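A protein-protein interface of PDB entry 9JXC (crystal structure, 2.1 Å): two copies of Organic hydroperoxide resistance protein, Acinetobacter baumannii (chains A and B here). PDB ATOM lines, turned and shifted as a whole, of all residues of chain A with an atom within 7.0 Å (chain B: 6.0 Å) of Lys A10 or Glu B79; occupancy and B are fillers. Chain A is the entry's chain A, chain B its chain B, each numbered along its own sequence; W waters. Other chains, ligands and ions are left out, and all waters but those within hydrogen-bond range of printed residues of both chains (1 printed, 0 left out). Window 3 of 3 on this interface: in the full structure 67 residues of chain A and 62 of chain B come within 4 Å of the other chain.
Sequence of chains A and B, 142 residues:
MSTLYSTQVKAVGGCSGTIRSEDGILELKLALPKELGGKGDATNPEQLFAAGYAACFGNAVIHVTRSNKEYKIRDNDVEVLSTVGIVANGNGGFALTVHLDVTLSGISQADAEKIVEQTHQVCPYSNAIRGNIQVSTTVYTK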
ATOM      1  N   GLN A   8       3.153  -6.616  16.691  1.00  0.00           N
ATOM      2  CA  GLN A   8       1.740  -6.724  17.116  1.00  0.00           C
ATOM      3  C   GLN A   8       1.697  -6.618  18.631  1.00  0.00           C
ATOM      4  O   GLN A   8       2.495  -7.320  19.321  1.00  0.00           O
ATOM      5  CB  GLN A   8       1.098  -8.035  16.662  1.00  0.00           C
ATOM      6  CG  GLN A   8       1.267  -8.319  15.181  1.00  0.00           C
ATOM      7  CD  GLN A   8       0.756  -9.698  14.823  1.00  0.00           C
ATOM      8  OE1 GLN A   8      -0.320 -10.103  15.227  1.00  0.00           O
ATOM      9  NE2 GLN A   8       1.535 -10.435  14.052  1.00  0.00           N
ATOM     10  N   VAL A   9       0.806  -5.773  19.129  1.00  0.00           N
ATOM     11  CA  VAL A   9       0.569  -5.634  20.586  1.00  0.00           C
ATOM     12  C   VAL A   9      -0.927  -5.797  20.834  1.00  0.00           C
ATOM     13  O   VAL A   9      -1.744  -5.212  20.068  1.00  0.00           O
ATOM     14  CB  VAL A   9       1.151  -4.323  21.139  1.00  0.00           C
ATOM     15  CG1 VAL A   9       1.005  -4.240  22.649  1.00  0.00           C
ATOM     16  CG2 VAL A   9       2.616  -4.197  20.750  1.00  0.00           C
ATOM     17  N   LYS A  10      -1.240  -6.628  21.827  1.00  0.00           N
ATOM     18  CA  LYS A  10      -2.616  -6.896  22.305  1.00  0.00           C
ATOM     19  C   LYS A  10      -2.833  -6.079  23.572  1.00  0.00           C
ATOM     20  O   LYS A  10      -1.942  -6.106  24.413  1.00  0.00           O
ATOM     21  CB  LYS A  10      -2.824  -8.382  22.600  1.00  0.00           C
ATOM     22  CG  LYS A  10      -4.234  -8.714  23.087  1.00  0.00           C
ATOM     23  CD  LYS A  10      -4.482 -10.175  23.373  1.00  0.00           C
ATOM     24  CE  LYS A  10      -4.299 -11.050  22.156  1.00  0.00           C
ATOM     25  NZ  LYS A  10      -4.456 -12.480  22.522  1.00  0.00           N
ATOM     26  N   ALA A  11      -3.947  -5.350  23.655  1.00  0.00           N
ATOM     27  CA  ALA A  11      -4.389  -4.608  24.850  1.00  0.00           C
ATOM     28  C   ALA A  11      -5.743  -5.156  25.290  1.00  0.00           C
ATOM     29  O   ALA A  11      -6.649  -5.251  24.432  1.00  0.00           O
ATOM     30  CB  ALA A  11      -4.466  -3.132  24.574  1.00  0.00           C
ATOM     31  N   VAL A  12      -5.852  -5.492  26.571  1.00  0.00           N
ATOM     32  CA  VAL A  12      -7.088  -6.027  27.221  1.00  0.00           C
ATOM     33  C   VAL A  12      -7.274  -5.279  28.555  1.00  0.00           C
ATOM     34  O   VAL A  12      -6.284  -4.695  29.058  1.00  0.00           O
ATOM     35  CB  VAL A  12      -6.970  -7.561  27.356  1.00  0.00           C
ATOM     36  CG1 VAL A  12      -5.939  -7.976  28.399  1.00  0.00           C
ATOM     37  CG2 VAL A  12      -8.312  -8.222  27.630  1.00  0.00           C
ATOM     38  N   GLY A  13      -8.509  -5.185  29.059  1.00  0.00           N
ATOM     39  CA  GLY A  13      -8.804  -4.831  30.456  1.00  0.00           C
ATOM     40  C   GLY A  13      -8.962  -3.338  30.676  1.00  0.00           C
ATOM     41  O   GLY A  13      -9.089  -2.936  31.844  1.00  0.00           O
ATOM     42  N   THR A  18      -3.721  -4.321  30.470  1.00  0.00           N
ATOM     43  CA  THR A  18      -2.351  -4.747  30.084  1.00  0.00           C
ATOM     44  C   THR A  18      -2.173  -4.629  28.570  1.00  0.00           C
ATOM     45  O   THR A  18      -3.203  -4.679  27.836  1.00  0.00           O
ATOM     46  CB  THR A  18      -2.038  -6.203  30.485  1.00  0.00           C
ATOM     47  OG1 THR A  18      -2.930  -7.043  29.749  1.00  0.00           O
ATOM     48  CG2 THR A  18      -2.156  -6.468  31.972  1.00  0.00           C
ATOM     49  N   ILE A  19      -0.913  -4.484  28.154  1.00  0.00           N
ATOM     50  CA  ILE A  19      -0.433  -4.659  26.757  1.00  0.00           C
ATOM     51  C   ILE A  19       0.650  -5.727  26.754  1.00  0.00           C
ATOM     52  O   ILE A  19       1.430  -5.806  27.721  1.00  0.00           O
ATOM     53  CB  ILE A  19       0.105  -3.357  26.141  1.00  0.00           C
ATOM     54  CG1 ILE A  19       1.360  -2.873  26.875  1.00  0.00           C
ATOM     55  CG2 ILE A  19      -1.012  -2.322  26.037  1.00  0.00           C
ATOM     56  CD1 ILE A  19       1.520  -1.383  26.951  1.00  0.00           C
ATOM     57  N   ARG A  20       0.728  -6.466  25.662  1.00  0.00           N
ATOM     58  CA  ARG A  20       1.727  -7.547  25.509  1.00  0.00           C
ATOM     59  C   ARG A  20       1.997  -7.696  24.025  1.00  0.00           C
ATOM     60  O   ARG A  20       1.036  -7.938  23.289  1.00  0.00           O
ATOM     61  CB  ARG A  20       1.191  -8.836  26.139  1.00  0.00           C
ATOM     62  CG  ARG A  20       2.237  -9.923  26.314  1.00  0.00           C
ATOM     63  CD  ARG A  20       1.609 -11.265  26.627  1.00  0.00           C
ATOM     64  NE  ARG A  20       2.634 -12.258  26.367  1.00  0.00           N
ATOM     65  CZ  ARG A  20       2.883 -12.824  25.185  1.00  0.00           C
ATOM     66  NH1 ARG A  20       2.157 -12.534  24.118  1.00  0.00           N
ATOM     67  NH2 ARG A  20       3.866 -13.703  25.079  1.00  0.00           N
ATOM     68  N   SER A  21       3.236  -7.466  23.610  1.00  0.00           N
ATOM     69  CA  SER A  21       3.696  -7.767  22.239  1.00  0.00           C
ATOM     70  C   SER A  21       3.606  -9.280  22.061  1.00  0.00           C
ATOM     71  O   SER A  21       3.672 -10.010  23.093  1.00  0.00           O
ATOM     72  CB  SER A  21       5.062  -7.236  21.935  1.00  0.00           C
ATOM     73  OG  SER A  21       6.024  -7.855  22.764  1.00  0.00           O
ATOM     74  N   GLU A  22       3.359  -9.710  20.822  1.00  0.00           N
ATOM     75  CA  GLU A  22       3.128 -11.133  20.471  1.00  0.00           C
ATOM     76  C   GLU A  22       4.436 -11.897  20.715  1.00  0.00           C
ATOM     77  O   GLU A  22       4.345 -13.004  21.201  1.00  0.00           O
ATOM     78  CB  GLU A  22       2.567 -11.242  19.051  1.00  0.00           C
ATOM     79  CG  GLU A  22       1.081 -10.888  18.950  1.00  0.00           C
ATOM     80  CD  GLU A  22       0.121 -11.799  19.710  1.00  0.00           C
ATOM     81  OE1 GLU A  22       0.406 -13.011  19.801  1.00  0.00           O
ATOM     82  OE2 GLU A  22      -0.897 -11.292  20.225  1.00  0.00           O
ATOM     83  N   ALA B  54      -3.212   0.397  20.772  1.00  0.00           N
ATOM     84  CA  ALA B  54      -4.067  -0.745  21.177  1.00  0.00           C
ATOM     85  C   ALA B  54      -4.801  -0.379  22.465  1.00  0.00           C
ATOM     86  O   ALA B  54      -6.010  -0.538  22.486  1.00  0.00           O
ATOM     87  CB  ALA B  54      -3.248  -1.985  21.325  1.00  0.00           C
ATOM     88  N   ASP B  75     -15.293  -2.957  30.035  1.00  0.00           N
ATOM     89  CA  ASP B  75     -13.826  -3.037  29.767  1.00  0.00           C
ATOM     90  C   ASP B  75     -13.411  -4.444  29.314  1.00  0.00           C
ATOM     91  O   ASP B  75     -12.637  -4.561  28.346  1.00  0.00           O
ATOM     92  CB  ASP B  75     -13.035  -2.636  31.006  1.00  0.00           C
ATOM     93  CG  ASP B  75     -13.046  -1.132  31.161  1.00  0.00           C
ATOM     94  OD1 ASP B  75     -12.507  -0.477  30.258  1.00  0.00           O
ATOM     95  OD2 ASP B  75     -13.672  -0.638  32.124  1.00  0.00           O
ATOM     96  N   ASP B  77     -15.037  -6.681  27.801  1.00  0.00           N
ATOM     97  CA  ASP B  77     -15.644  -7.091  26.507  1.00  0.00           C
ATOM     98  C   ASP B  77     -14.788  -6.571  25.342  1.00  0.00           C
ATOM     99  O   ASP B  77     -15.143  -6.857  24.185  1.00  0.00           O
ATOM    100  CB  ASP B  77     -17.107  -6.626  26.430  1.00  0.00           C
ATOM    101  CG  ASP B  77     -17.976  -7.224  27.533  1.00  0.00           C
ATOM    102  OD1 ASP B  77     -17.699  -8.385  27.935  1.00  0.00           O
ATOM    103  OD2 ASP B  77     -18.881  -6.511  28.017  1.00  0.00           O
ATOM    104  N   VAL B  78     -13.697  -5.843  25.608  1.00  0.00           N
ATOM    105  CA  VAL B  78     -12.949  -5.136  24.528  1.00  0.00           C
ATOM    106  C   VAL B  78     -11.518  -5.670  24.443  1.00  0.00           C
ATOM    107  O   VAL B  78     -10.785  -5.612  25.435  1.00  0.00           O
ATOM    108  CB  VAL B  78     -12.952  -3.606  24.728  1.00  0.00           C
ATOM    109  CG1 VAL B  78     -12.220  -2.918  23.581  1.00  0.00           C
ATOM    110  CG2 VAL B  78     -14.365  -3.061  24.871  1.00  0.00           C
ATOM    111  N   GLU B  79     -11.110  -6.076  23.257  1.00  0.00           N
ATOM    112  CA  GLU B  79      -9.720  -6.499  22.975  1.00  0.00           C
ATOM    113  C   GLU B  79      -9.262  -5.813  21.692  1.00  0.00           C
ATOM    114  O   GLU B  79     -10.033  -5.809  20.724  1.00  0.00           O
ATOM    115  CB  GLU B  79      -9.693  -8.023  22.899  1.00  0.00           C
ATOM    116  CG  GLU B  79      -8.306  -8.607  22.758  1.00  0.00           C
ATOM    117  CD  GLU B  79      -8.320 -10.124  22.846  1.00  0.00           C
ATOM    118  OE1 GLU B  79      -8.921 -10.643  23.810  1.00  0.00           O
ATOM    119  OE2 GLU B  79      -7.764 -10.776  21.941  1.00  0.00           O
ATOM    120  N   VAL B  80      -8.068  -5.224  21.693  1.00  0.00           N
ATOM    121  CA  VAL B  80      -7.454  -4.607  20.477  1.00  0.00           C
ATOM    122  C   VAL B  80      -6.067  -5.207  20.237  1.00  0.00           C
ATOM    123  O   VAL B  80      -5.252  -5.246  21.170  1.00  0.00           O
ATOM    124  CB  VAL B  80      -7.377  -3.077  20.574  1.00  0.00           C
ATOM    125  CG1 VAL B  80      -6.850  -2.458  19.296  1.00  0.00           C
ATOM    126  CG2 VAL B  80      -8.715  -2.476  20.901  1.00  0.00           C
ATOM    127  N   LEU B  81      -5.830  -5.629  18.995  1.00  0.00           N
ATOM    128  CA  LEU B  81      -4.524  -6.058  18.463  1.00  0.00           C
ATOM    129  C   LEU B  81      -4.104  -5.033  17.419  1.00  0.00           C
ATOM    130  O   LEU B  81      -4.820  -4.887  16.406  1.00  0.00           O
ATOM    131  CB  LEU B  81      -4.638  -7.468  17.871  1.00  0.00           C
ATOM    132  CG  LEU B  81      -3.328  -8.081  17.386  1.00  0.00           C
ATOM    133  CD1 LEU B  81      -2.462  -8.507  18.570  1.00  0.00           C
ATOM    134  CD2 LEU B  81      -3.608  -9.260  16.477  1.00  0.00           C
ATOM    135  N   SER B  82      -3.060  -4.264  17.710  1.00  0.00           N
ATOM    136  CA  SER B  82      -2.471  -3.307  16.748  1.00  0.00           C
ATOM    137  C   SER B  82      -1.316  -4.017  16.064  1.00  0.00           C
ATOM    138  O   SER B  82      -0.508  -4.665  16.781  1.00  0.00           O
ATOM    139  CB  SER B  82      -1.987  -2.069  17.393  1.00  0.00           C
ATOM    140  OG  SER B  82      -1.002  -2.443  18.321  1.00  0.00           O
ATOM    141  N   ASP B 101      -7.128  -5.079  14.833  1.00  0.00           N
ATOM    142  CA  ASP B 101      -8.183  -6.106  15.043  1.00  0.00           C
ATOM    143  C   ASP B 101      -8.883  -5.798  16.364  1.00  0.00           C
ATOM    144  O   ASP B 101      -8.230  -5.885  17.435  1.00  0.00           O
ATOM    145  CB  ASP B 101      -7.622  -7.522  14.949  1.00  0.00           C
ATOM    146  CG  ASP B 101      -6.995  -7.776  13.592  1.00  0.00           C
ATOM    147  OD1 ASP B 101      -7.652  -7.521  12.600  1.00  0.00           O
ATOM    148  OD2 ASP B 101      -5.845  -8.154  13.560  1.00  0.00           O
ATOM    149  N   VAL B 102     -10.141  -5.385  16.267  1.00  0.00           N
ATOM    150  CA  VAL B 102     -10.988  -5.045  17.437  1.00  0.00           C
ATOM    151  C   VAL B 102     -11.963  -6.202  17.642  1.00  0.00           C
ATOM    152  O   VAL B 102     -12.825  -6.422  16.733  1.00  0.00           O
ATOM    153  CB  VAL B 102     -11.737  -3.711  17.223  1.00  0.00           C
ATOM    154  CG1 VAL B 102     -12.488  -3.264  18.484  1.00  0.00           C
ATOM    155  CG2 VAL B 102     -10.800  -2.608  16.728  1.00  0.00           C
ATOM    156  N   THR B 103     -11.910  -6.850  18.807  1.00  0.00           N
ATOM    157  CA  THR B 103     -12.882  -7.897  19.217  1.00  0.00           C
ATOM    158  C   THR B 103     -13.760  -7.347  20.360  1.00  0.00           C
ATOM    159  O   THR B 103     -13.221  -6.944  21.402  1.00  0.00           O
ATOM    160  CB  THR B 103     -12.109  -9.192  19.487  1.00  0.00           C
ATOM    161  OG1 THR B 103     -11.398  -9.504  18.280  1.00  0.00           O
ATOM    162  CG2 THR B 103     -13.002 -10.326  19.945  1.00  0.00           C
ATOM    163  N   LEU B 104     -15.069  -7.258  20.124  1.00  0.00           N
ATOM    164  CA  LEU B 104     -16.081  -6.823  21.112  1.00  0.00           C
ATOM    165  C   LEU B 104     -16.991  -8.017  21.431  1.00  0.00           C
ATOM    166  O   LEU B 104     -17.535  -8.636  20.461  1.00  0.00           O
ATOM    167  CB  LEU B 104     -16.870  -5.651  20.531  1.00  0.00           C
ATOM    168  CG  LEU B 104     -16.019  -4.491  20.007  1.00  0.00           C
ATOM    169  CD1 LEU B 104     -16.902  -3.391  19.473  1.00  0.00           C
ATOM    170  CD2 LEU B 104     -15.113  -3.916  21.095  1.00  0.00           C
HETATM  171  O   HOH W   1     -10.107  -3.172  26.849  1.00  0.00           O
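N of Thr B103 is in hydrogen-bond range of O of Glu B79 (2.9 Å). O of Leu B81 lies within hydrogen-bond range of N of Asp B101 (2.8 Å). The backbone carbonyl oxygen (O) of Gln A8 sits at hydrogen-bond distance from the backbone NH (N) of Glu A22 (3.0 Å). N of Arg A20 lies within hydrogen-bond range of O of Lys A10 (3.0 Å).
Lys A10 touches three residues of chain B. Of the printed residues of chain B, Ala A11 touches Ala B54, Glu B79 and Val B80. Gly A13 touches none of the printed residues of chain B. Of the printed residues of chain A, Val B80 touches Val A9 (3.7 Å), Lys A10 (3.3 Å) and Ala A11 (2.8 Å). The nearest residue of chain B that does not touch Lys A10 is Ala B54 (4.7 Å). The nearest printed residue of chain A that does not touch Leu B81 is Ala A11 (5.0 Å).
Among the printed residues, pairs that only touch across the chains: Gln A8 with Leu B81 (3.6 Å), Gln A8 with Ser B82 (3.1 Å), Val A9 with Ala B54 (3.8 Å), Val A9 with Val B80 (3.7 Å), Val A9 with Leu B81 (3.3 Å), Lys A10 with Val B80 (3.3 Å), Lys A10 with Leu B81 (3.95 Å), Ala A11 with Ala B54 (3.5 Å), Ala A11 with Glu B79 (3.6 Å) and Glu A22 with Leu B81 (3.6 Å).
Water W1 lies within hydrogen-bond range of O of Val B78, O of Asp B75 and N of Gly A13.
No position is printed for both chains. Of the 13 pairs that touch across the chains among the printed residues, none has its exchanged pair printed and touching as well.
Of the 12 printed residues of chain B, 5 touch a printed residue of chain A. Hydrophobic or aromatic side chains of chain B that line the printed part of chain A: Ala B54 and Leu B81. Along chain B the printed residues that touch a printed residue of chain A span positions 54 to 82. Of the 11 printed residues of chain A, 5 touch a printed residue of chain B. Hydrophobic or aromatic side chains of chain A that line the printed part of chain B: Ala A11.
The side-chain amino group (NZ) of Lys A10 lies within salt-bridge range of the side-chain carboxylate (OE2) of Glu B79, 3.8 Å away. O of Val B80 is in hydrogen-bond range of N of Ala A11 (2.8 Å). O of Val A9 is in hydrogen-bond range of N of Ser B82, at 2.9 Å.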
